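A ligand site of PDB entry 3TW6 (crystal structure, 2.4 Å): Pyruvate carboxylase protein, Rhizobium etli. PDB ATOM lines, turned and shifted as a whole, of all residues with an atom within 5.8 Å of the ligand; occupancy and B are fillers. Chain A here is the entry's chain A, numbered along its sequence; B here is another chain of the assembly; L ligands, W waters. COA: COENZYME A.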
ATOM      1  N   ARG A 438     -18.307 -21.964 -20.015  1.00  0.00           N
ATOM      2  CA  ARG A 438     -17.898 -20.695 -19.421  1.00  0.00           C
ATOM      3  C   ARG A 438     -19.067 -20.067 -18.672  1.00  0.00           C
ATOM      4  O   ARG A 438     -20.083 -19.669 -19.253  1.00  0.00           O
ATOM      5  CB  ARG A 438     -17.319 -19.681 -20.428  1.00  0.00           C
ATOM      6  CG  ARG A 438     -16.010 -20.103 -21.094  1.00  0.00           C
ATOM      7  CD  ARG A 438     -14.838 -20.405 -20.147  1.00  0.00           C
ATOM      8  NE  ARG A 438     -13.663 -20.937 -20.836  1.00  0.00           N
ATOM      9  CZ  ARG A 438     -13.423 -22.240 -20.974  1.00  0.00           C
ATOM     10  NH1 ARG A 438     -14.277 -23.092 -20.454  1.00  0.00           N
ATOM     11  NH2 ARG A 438     -12.330 -22.687 -21.608  1.00  0.00           N
ATOM     12  N   ARG A 440     -19.529 -17.020 -15.804  1.00  0.00           N
ATOM     13  CA  ARG A 440     -18.937 -15.936 -15.010  1.00  0.00           C
ATOM     14  C   ARG A 440     -19.965 -15.087 -14.273  1.00  0.00           C
ATOM     15  O   ARG A 440     -21.097 -14.835 -14.740  1.00  0.00           O
ATOM     16  CB  ARG A 440     -18.032 -15.014 -15.836  1.00  0.00           C
ATOM     17  CG  ARG A 440     -16.794 -15.658 -16.487  1.00  0.00           C
ATOM     18  CD  ARG A 440     -15.704 -16.134 -15.513  1.00  0.00           C
ATOM     19  NE  ARG A 440     -14.580 -16.826 -16.199  1.00  0.00           N
ATOM     20  CZ  ARG A 440     -14.539 -18.129 -16.509  1.00  0.00           C
ATOM     21  NH1 ARG A 440     -15.533 -18.949 -16.218  1.00  0.00           N
ATOM     22  NH2 ARG A 440     -13.468 -18.630 -17.115  1.00  0.00           N
ATOM     23  N   ARG A 480      -6.571 -20.336 -10.192  1.00  0.00           N
ATOM     24  CA  ARG A 480      -6.836 -19.926 -11.588  1.00  0.00           C
ATOM     25  C   ARG A 480      -5.928 -18.696 -11.901  1.00  0.00           C
ATOM     26  O   ARG A 480      -5.739 -17.835 -11.053  1.00  0.00           O
ATOM     27  CB  ARG A 480      -8.332 -19.595 -11.788  1.00  0.00           C
ATOM     28  CG  ARG A 480      -8.963 -20.134 -13.092  1.00  0.00           C
ATOM     29  CD  ARG A 480     -10.401 -19.640 -13.362  1.00  0.00           C
ATOM     30  NE  ARG A 480     -10.559 -18.177 -13.323  1.00  0.00           N
ATOM     31  CZ  ARG A 480     -10.550 -17.355 -14.376  1.00  0.00           C
ATOM     32  NH1 ARG A 480     -10.393 -17.808 -15.620  1.00  0.00           N
ATOM     33  NH2 ARG A 480     -10.688 -16.046 -14.195  1.00  0.00           N
ATOM     34  N   GLN A 481      -5.357 -18.622 -13.101  1.00  0.00           N
ATOM     35  CA  GLN A 481      -4.394 -17.556 -13.427  1.00  0.00           C
ATOM     36  C   GLN A 481      -5.043 -16.189 -13.671  1.00  0.00           C
ATOM     37  O   GLN A 481      -4.532 -15.153 -13.221  1.00  0.00           O
ATOM     38  CB  GLN A 481      -3.576 -17.946 -14.668  1.00  0.00           C
ATOM     39  CG  GLN A 481      -2.660 -19.149 -14.468  1.00  0.00           C
ATOM     40  CD  GLN A 481      -2.083 -19.639 -15.778  1.00  0.00           C
ATOM     41  OE1 GLN A 481      -0.889 -19.457 -16.025  1.00  0.00           O
ATOM     42  NE2 GLN A 481      -2.914 -20.245 -16.638  1.00  0.00           N
ATOM     43  N   ASP A 482      -6.139 -16.196 -14.442  1.00  0.00           N
ATOM     44  CA  ASP A 482      -6.833 -14.969 -14.687  1.00  0.00           C
ATOM     45  C   ASP A 482      -5.902 -13.862 -15.267  1.00  0.00           C
ATOM     46  O   ASP A 482      -5.883 -12.698 -14.818  1.00  0.00           O
ATOM     47  CB  ASP A 482      -7.456 -14.552 -13.363  1.00  0.00           C
ATOM     48  CG  ASP A 482      -8.299 -13.346 -13.501  1.00  0.00           C
ATOM     49  OD1 ASP A 482      -8.264 -12.516 -12.550  1.00  0.00           O
ATOM     50  OD2 ASP A 482      -8.953 -13.230 -14.577  1.00  0.00           O
ATOM     51  N   ARG A 483      -5.142 -14.264 -16.275  1.00  0.00           N
ATOM     52  CA  ARG A 483      -4.143 -13.426 -16.849  1.00  0.00           C
ATOM     53  C   ARG A 483      -4.667 -12.192 -17.555  1.00  0.00           C
ATOM     54  O   ARG A 483      -4.089 -11.132 -17.356  1.00  0.00           O
ATOM     55  CB  ARG A 483      -3.142 -14.246 -17.679  1.00  0.00           C
ATOM     56  CG  ARG A 483      -2.126 -14.951 -16.746  1.00  0.00           C
ATOM     57  CD  ARG A 483      -1.151 -15.840 -17.487  1.00  0.00           C
ATOM     58  NE  ARG A 483      -1.873 -16.951 -18.070  1.00  0.00           N
ATOM     59  CZ  ARG A 483      -1.402 -17.784 -18.994  1.00  0.00           C
ATOM     60  NH1 ARG A 483      -0.175 -17.659 -19.472  1.00  0.00           N
ATOM     61  NH2 ARG A 483      -2.176 -18.752 -19.451  1.00  0.00           N
ATOM     62  N   ALA A 484      -5.764 -12.330 -18.313  1.00  0.00           N
ATOM     63  CA  ALA A 484      -6.356 -11.235 -19.103  1.00  0.00           C
ATOM     64  C   ALA A 484      -6.729 -10.070 -18.179  1.00  0.00           C
ATOM     65  O   ALA A 484      -6.365  -8.920 -18.443  1.00  0.00           O
ATOM     66  CB  ALA A 484      -7.610 -11.704 -19.834  1.00  0.00           C
ATOM     67  N   ILE A1037      -1.006 -13.557 -24.530  1.00  0.00           N
ATOM     68  CA  ILE A1037      -0.799 -14.021 -23.164  1.00  0.00           C
ATOM     69  C   ILE A1037       0.143 -15.244 -23.189  1.00  0.00           C
ATOM     70  O   ILE A1037       0.891 -15.499 -22.250  1.00  0.00           O
ATOM     71  CB  ILE A1037      -2.176 -14.246 -22.423  1.00  0.00           C
ATOM     72  N   GLU A1038       0.117 -15.978 -24.292  1.00  0.00           N
ATOM     73  CA  GLU A1038       0.985 -17.154 -24.513  1.00  0.00           C
ATOM     74  C   GLU A1038       1.038 -17.397 -25.989  1.00  0.00           C
ATOM     75  O   GLU A1038       0.167 -16.912 -26.693  1.00  0.00           O
ATOM     76  CB  GLU A1038       0.307 -18.398 -23.998  1.00  0.00           C
ATOM     77  CG  GLU A1038       0.624 -18.824 -22.599  1.00  0.00           C
ATOM     78  CD  GLU A1038      -0.201 -20.056 -22.308  1.00  0.00           C
ATOM     79  OE1 GLU A1038      -0.166 -20.979 -23.137  1.00  0.00           O
ATOM     80  OE2 GLU A1038      -0.918 -20.072 -21.292  1.00  0.00           O
ATOM     81  N   GLY A1040      -0.118 -18.577 -29.054  1.00  0.00           N
ATOM     82  CA  GLY A1040      -1.385 -19.195 -29.477  1.00  0.00           C
ATOM     83  C   GLY A1040      -2.641 -18.929 -28.643  1.00  0.00           C
ATOM     84  O   GLY A1040      -3.664 -19.584 -28.888  1.00  0.00           O
ATOM     85  N   LYS A1041      -2.524 -18.009 -27.665  1.00  0.00           N
ATOM     86  CA  LYS A1041      -3.619 -17.433 -26.911  1.00  0.00           C
ATOM     87  C   LYS A1041      -3.555 -15.887 -27.083  1.00  0.00           C
ATOM     88  O   LYS A1041      -2.950 -15.177 -26.257  1.00  0.00           O
ATOM     89  CB  LYS A1041      -3.616 -17.874 -25.418  1.00  0.00           C
ATOM     90  N   THR A1042      -4.192 -15.385 -28.160  1.00  0.00           N
ATOM     91  CA  THR A1042      -4.246 -13.968 -28.521  1.00  0.00           C
ATOM     92  C   THR A1042      -5.542 -13.303 -28.003  1.00  0.00           C
ATOM     93  O   THR A1042      -6.676 -13.725 -28.379  1.00  0.00           O
ATOM     94  CB  THR A1042      -4.215 -13.800 -30.057  1.00  0.00           C
ATOM     95  OG1 THR A1042      -2.938 -14.227 -30.518  1.00  0.00           O
ATOM     96  CG2 THR A1042      -4.414 -12.328 -30.515  1.00  0.00           C
ATOM     97  N   LEU A1043      -5.352 -12.323 -27.129  1.00  0.00           N
ATOM     98  CA  LEU A1043      -6.396 -11.401 -26.668  1.00  0.00           C
ATOM     99  C   LEU A1043      -6.509 -10.217 -27.586  1.00  0.00           C
ATOM    100  O   LEU A1043      -5.486  -9.656 -28.002  1.00  0.00           O
ATOM    101  CB  LEU A1043      -6.037 -10.833 -25.295  1.00  0.00           C
ATOM    102  CG  LEU A1043      -5.692 -11.851 -24.200  1.00  0.00           C
ATOM    103  CD1 LEU A1043      -5.485 -11.173 -22.855  1.00  0.00           C
ATOM    104  CD2 LEU A1043      -6.798 -12.889 -24.081  1.00  0.00           C
ATOM    105  N   LEU A1065     -12.636  -6.819 -24.408  1.00  0.00           N
ATOM    106  CA  LEU A1065     -11.731  -7.962 -24.403  1.00  0.00           C
ATOM    107  C   LEU A1065     -12.362  -9.088 -25.226  1.00  0.00           C
ATOM    108  O   LEU A1065     -13.331  -9.726 -24.801  1.00  0.00           O
ATOM    109  CB  LEU A1065     -11.533  -8.471 -22.987  1.00  0.00           C
ATOM    110  CG  LEU A1065     -10.597  -9.684 -22.785  1.00  0.00           C
ATOM    111  CD1 LEU A1065      -9.167  -9.319 -23.172  1.00  0.00           C
ATOM    112  CD2 LEU A1065     -10.633 -10.278 -21.378  1.00  0.00           C
ATOM    113  N   ASN A1066     -11.839  -9.301 -26.431  1.00  0.00           N
ATOM    114  CA  ASN A1066     -12.331 -10.362 -27.285  1.00  0.00           C
ATOM    115  C   ASN A1066     -13.795 -10.133 -27.556  1.00  0.00           C
ATOM    116  O   ASN A1066     -14.546 -11.071 -27.541  1.00  0.00           O
ATOM    117  CB  ASN A1066     -12.061 -11.738 -26.639  1.00  0.00           C
ATOM    118  CG  ASN A1066     -10.577 -12.133 -26.685  1.00  0.00           C
ATOM    119  OD1 ASN A1066      -9.809 -11.595 -27.500  1.00  0.00           O
ATOM    120  ND2 ASN A1066     -10.177 -13.100 -25.871  1.00  0.00           N
ATOM    121  N   ARG A1070     -15.486  -4.932 -20.440  1.00  0.00           N
ATOM    122  CA  ARG A1070     -14.875  -5.160 -19.134  1.00  0.00           C
ATOM    123  C   ARG A1070     -14.522  -3.794 -18.575  1.00  0.00           C
ATOM    124  O   ARG A1070     -13.954  -2.954 -19.272  1.00  0.00           O
ATOM    125  CB  ARG A1070     -13.617  -6.023 -19.247  1.00  0.00           C
ATOM    126  CG  ARG A1070     -13.746  -7.332 -20.015  1.00  0.00           C
ATOM    127  CD  ARG A1070     -14.545  -8.331 -19.192  1.00  0.00           C
ATOM    128  NE  ARG A1070     -14.033  -8.255 -17.836  1.00  0.00           N
ATOM    129  CZ  ARG A1070     -13.119  -9.089 -17.330  1.00  0.00           C
ATOM    130  NH1 ARG A1070     -12.662 -10.126 -18.035  1.00  0.00           N
ATOM    131  NH2 ARG A1070     -12.692  -8.879 -16.087  1.00  0.00           N
ATOM    132  N   ARG B  54     -12.312 -19.746 -32.853  1.00  0.00           N
ATOM    133  CA  ARG B  54     -10.917 -19.585 -32.482  1.00  0.00           C
ATOM    134  C   ARG B  54     -10.583 -19.716 -30.967  1.00  0.00           C
ATOM    135  O   ARG B  54      -9.435 -19.973 -30.595  1.00  0.00           O
ATOM    136  CB  ARG B  54     -10.324 -18.273 -33.048  1.00  0.00           C
ATOM    137  CG  ARG B  54     -10.546 -17.019 -32.181  1.00  0.00           C
ATOM    138  CD  ARG B  54      -9.471 -16.072 -32.540  1.00  0.00           C
ATOM    139  NE  ARG B  54      -9.410 -14.787 -31.854  1.00  0.00           N
ATOM    140  CZ  ARG B  54      -8.605 -14.487 -30.846  1.00  0.00           C
ATOM    141  NH1 ARG B  54      -7.862 -15.415 -30.269  1.00  0.00           N
ATOM    142  NH2 ARG B  54      -8.603 -13.237 -30.380  1.00  0.00           N
ATOM    143  N   PHE B  55     -11.571 -19.484 -30.093  1.00  0.00           N
ATOM    144  CA  PHE B  55     -11.339 -19.609 -28.661  1.00  0.00           C
ATOM    145  C   PHE B  55     -11.664 -21.039 -28.254  1.00  0.00           C
ATOM    146  O   PHE B  55     -11.529 -21.429 -27.105  1.00  0.00           O
ATOM    147  CB  PHE B  55     -12.177 -18.593 -27.880  1.00  0.00           C
ATOM    148  CG  PHE B  55     -11.986 -17.162 -28.331  1.00  0.00           C
ATOM    149  CD1 PHE B  55     -10.871 -16.430 -27.911  1.00  0.00           C
ATOM    150  CD2 PHE B  55     -12.902 -16.563 -29.198  1.00  0.00           C
ATOM    151  CE1 PHE B  55     -10.670 -15.137 -28.343  1.00  0.00           C
ATOM    152  CE2 PHE B  55     -12.722 -15.252 -29.617  1.00  0.00           C
ATOM    153  CZ  PHE B  55     -11.609 -14.531 -29.191  1.00  0.00           C
ATOM    154  N   LYS B  56     -12.059 -21.850 -29.229  1.00  0.00           N
ATOM    155  CA  LYS B  56     -12.501 -23.218 -28.912  1.00  0.00           C
ATOM    156  C   LYS B  56     -11.422 -24.293 -29.056  1.00  0.00           C
ATOM    157  O   LYS B  56     -11.656 -25.456 -28.774  1.00  0.00           O
ATOM    158  CB  LYS B  56     -13.828 -23.563 -29.663  1.00  0.00           C
ATOM    159  N   ALA B  57     -10.234 -23.899 -29.470  1.00  0.00           N
ATOM    160  CA  ALA B  57      -9.106 -24.815 -29.650  1.00  0.00           C
ATOM    161  C   ALA B  57      -8.090 -24.658 -28.521  1.00  0.00           C
ATOM    162  O   ALA B  57      -8.181 -23.724 -27.751  1.00  0.00           O
ATOM    163  CB  ALA B  57      -8.450 -24.587 -31.018  1.00  0.00           C
ATOM    164  N   ASP B  58      -7.133 -25.577 -28.415  1.00  0.00           N
ATOM    165  CA  ASP B  58      -6.116 -25.511 -27.334  1.00  0.00           C
ATOM    166  C   ASP B  58      -5.180 -24.338 -27.578  1.00  0.00           C
ATOM    167  O   ASP B  58      -4.617 -23.773 -26.656  1.00  0.00           O
ATOM    168  CB  ASP B  58      -5.315 -26.823 -27.195  1.00  0.00           C
ATOM    169  CG  ASP B  58      -6.195 -28.028 -26.813  1.00  0.00           C
ATOM    170  OD1 ASP B  58      -6.945 -27.966 -25.812  1.00  0.00           O
ATOM    171  OD2 ASP B  58      -6.149 -29.071 -27.527  1.00  0.00           O
ATOM    172  N   GLU B  59      -5.026 -23.952 -28.833  1.00  0.00           N
ATOM    173  CA  GLU B  59      -4.183 -22.834 -29.165  1.00  0.00           C
ATOM    174  C   GLU B  59      -4.655 -22.416 -30.539  1.00  0.00           C
ATOM    175  O   GLU B  59      -5.342 -23.181 -31.178  1.00  0.00           O
ATOM    176  CB  GLU B  59      -2.680 -23.275 -29.123  1.00  0.00           C
ATOM    177  CG  GLU B  59      -2.335 -24.549 -29.896  1.00  0.00           C
ATOM    178  CD  GLU B  59      -0.849 -24.926 -29.846  1.00  0.00           C
ATOM    179  OE1 GLU B  59      -0.004 -24.024 -29.656  1.00  0.00           O
ATOM    180  OE2 GLU B  59      -0.511 -26.115 -29.995  1.00  0.00           O
ATOM    181  N   SER B  60      -4.332 -21.204 -30.990  1.00  0.00           N
ATOM    182  CA  SER B  60      -4.849 -20.722 -32.260  1.00  0.00           C
ATOM    183  C   SER B  60      -4.000 -19.597 -32.834  1.00  0.00           C
ATOM    184  O   SER B  60      -3.403 -18.813 -32.098  1.00  0.00           O
ATOM    185  CB  SER B  60      -6.314 -20.242 -32.052  1.00  0.00           C
ATOM    186  OG  SER B  60      -6.486 -18.835 -32.244  1.00  0.00           O
HETATM  187  N1A COA L   1      -7.707 -17.481 -27.226  1.00  0.00           N
HETATM  188  C2A COA L   1      -7.872 -16.182 -26.876  1.00  0.00           C
HETATM  189  N3A COA L   1      -8.133 -15.734 -25.630  1.00  0.00           N
HETATM  190  C4A COA L   1      -8.235 -16.617 -24.601  1.00  0.00           C
HETATM  191  C5A COA L   1      -8.064 -18.057 -24.911  1.00  0.00           C
HETATM  192  C6A COA L   1      -7.791 -18.456 -26.317  1.00  0.00           C
HETATM  193  N6A COA L   1      -7.626 -19.738 -26.683  1.00  0.00           N
HETATM  194  N7A COA L   1      -8.210 -18.716 -23.735  1.00  0.00           N
HETATM  195  C8A COA L   1      -8.447 -17.793 -22.777  1.00  0.00           C
HETATM  196  N9A COA L   1      -8.461 -16.533 -23.279  1.00  0.00           N
HETATM  197  C1B COA L   1      -8.714 -15.275 -22.491  1.00  0.00           C
HETATM  198  C2B COA L   1     -10.024 -15.387 -21.699  1.00  0.00           C
HETATM  199  O2B COA L   1     -10.546 -14.144 -21.238  1.00  0.00           O
HETATM  200  C3B COA L   1      -9.505 -16.142 -20.496  1.00  0.00           C
HETATM  201  O3B COA L   1     -10.457 -16.349 -19.444  1.00  0.00           O
HETATM  202  P3B COA L   1     -11.136 -17.843 -19.440  1.00  0.00           P
HETATM  203  O7A COA L   1     -12.611 -17.459 -19.413  1.00  0.00           O
HETATM  204  O8A COA L   1     -10.734 -18.600 -20.715  1.00  0.00           O
HETATM  205  O9A COA L   1     -10.567 -18.548 -18.219  1.00  0.00           O
HETATM  206  C4B COA L   1      -8.133 -15.530 -20.202  1.00  0.00           C
HETATM  207  O4B COA L   1      -7.672 -15.140 -21.500  1.00  0.00           O
HETATM  208  C5B COA L   1      -7.200 -16.628 -19.786  1.00  0.00           C
HETATM  209  O5B COA L   1      -6.447 -16.267 -18.652  1.00  0.00           O
HETATM  210  P1A COA L   1      -5.623 -17.526 -18.119  1.00  0.00           P
HETATM  211  O1A COA L   1      -4.256 -17.092 -17.719  1.00  0.00           O
HETATM  212  O2A COA L   1      -5.858 -18.656 -19.121  1.00  0.00           O
HETATM  213  O3A COA L   1      -6.234 -17.768 -16.657  1.00  0.00           O
HETATM  214  P2A COA L   1      -6.947 -19.082 -16.072  1.00  0.00           P
HETATM  215  O4A COA L   1      -5.961 -20.080 -15.485  1.00  0.00           O
HETATM  216  O5A COA L   1      -7.803 -18.244 -15.161  1.00  0.00           O
HETATM  217  O6A COA L   1      -7.800 -19.741 -17.325  1.00  0.00           O
HETATM  218  CCP COA L   1      -8.491 -21.010 -17.316  1.00  0.00           C
HETATM  219  O   HOH W   1     -15.741 -16.732 -20.538  1.00  0.00           O
HETATM  220  O   HOH W   2      -7.352 -17.852 -29.629  1.00  0.00           O
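N of Arg 483 lies close to O1A of the ligand (3.3 Å). NE of Arg 483 is in salt-bridge range of O1A of the ligand, at 2.4 Å. An oxygen (O5A) of the ligand lies within salt-bridge range of the guanidinium group of Arg 480 (2.7 Å). O3A of the ligand is in hydrogen-bond range of N of Asp 482 (2.7 Å). An oxygen (O7A) of the ligand lies within salt-bridge range of the guanidinium group of Arg 440. N of Gln 481 sits at hydrogen-bond distance from O4A of the ligand (2.9 Å). O4A of the ligand is in hydrogen-bond range of NE2 of Gln 481 (3.3 Å). The side-chain amide nitrogen of Asn 1066 lies within hydrogen-bond range of a nitrogen (N3A) of the ligand (3.3 Å). An oxygen (O8A) of the ligand is in salt-bridge range of the guanidinium group (NE) of Arg 438.
Residues that only touch the ligand: Thr 1042, Phe 55 of chain B, Leu 1043, Arg 54 of chain B, Ala 484 and Leu 1065. Within 4 Å of the ligand: Arg 438, Arg 440, Arg 480, Gln 481, Asp 482, Arg 483, Ala 484, Thr 1042, Leu 1043, Leu 1065, Asn 1066, Arg 54 of chain B and Phe 55 of chain B. Along chain A the residues within 4 Å of the ligand span positions 438 to 1066. The nearest printed residue that does not touch the ligand is Lys 1041 (4.1 Å).
The guanidinium group of Arg 483 sits close to the side-chain amide nitrogen of Gln 481, 3.3 Å away. The guanidinium group (NH2) of Arg 483 lies within salt-bridge range of the side-chain carboxylate (OE2) of Glu 1038, 2.6 Å away. NH2 of Arg 480 lies within salt-bridge range of OD2 of Asp 482 (3.3 Å). NH1 of Arg 54 of chain B lies within hydrogen-bond range of O of Thr 1042 (2.8 Å).
Water W2 lies within hydrogen-bond range of a nitrogen (N1A) of the ligand, the guanidinium group of Arg 54 of chain B and the side-chain hydroxyl of Ser 60 of chain B.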
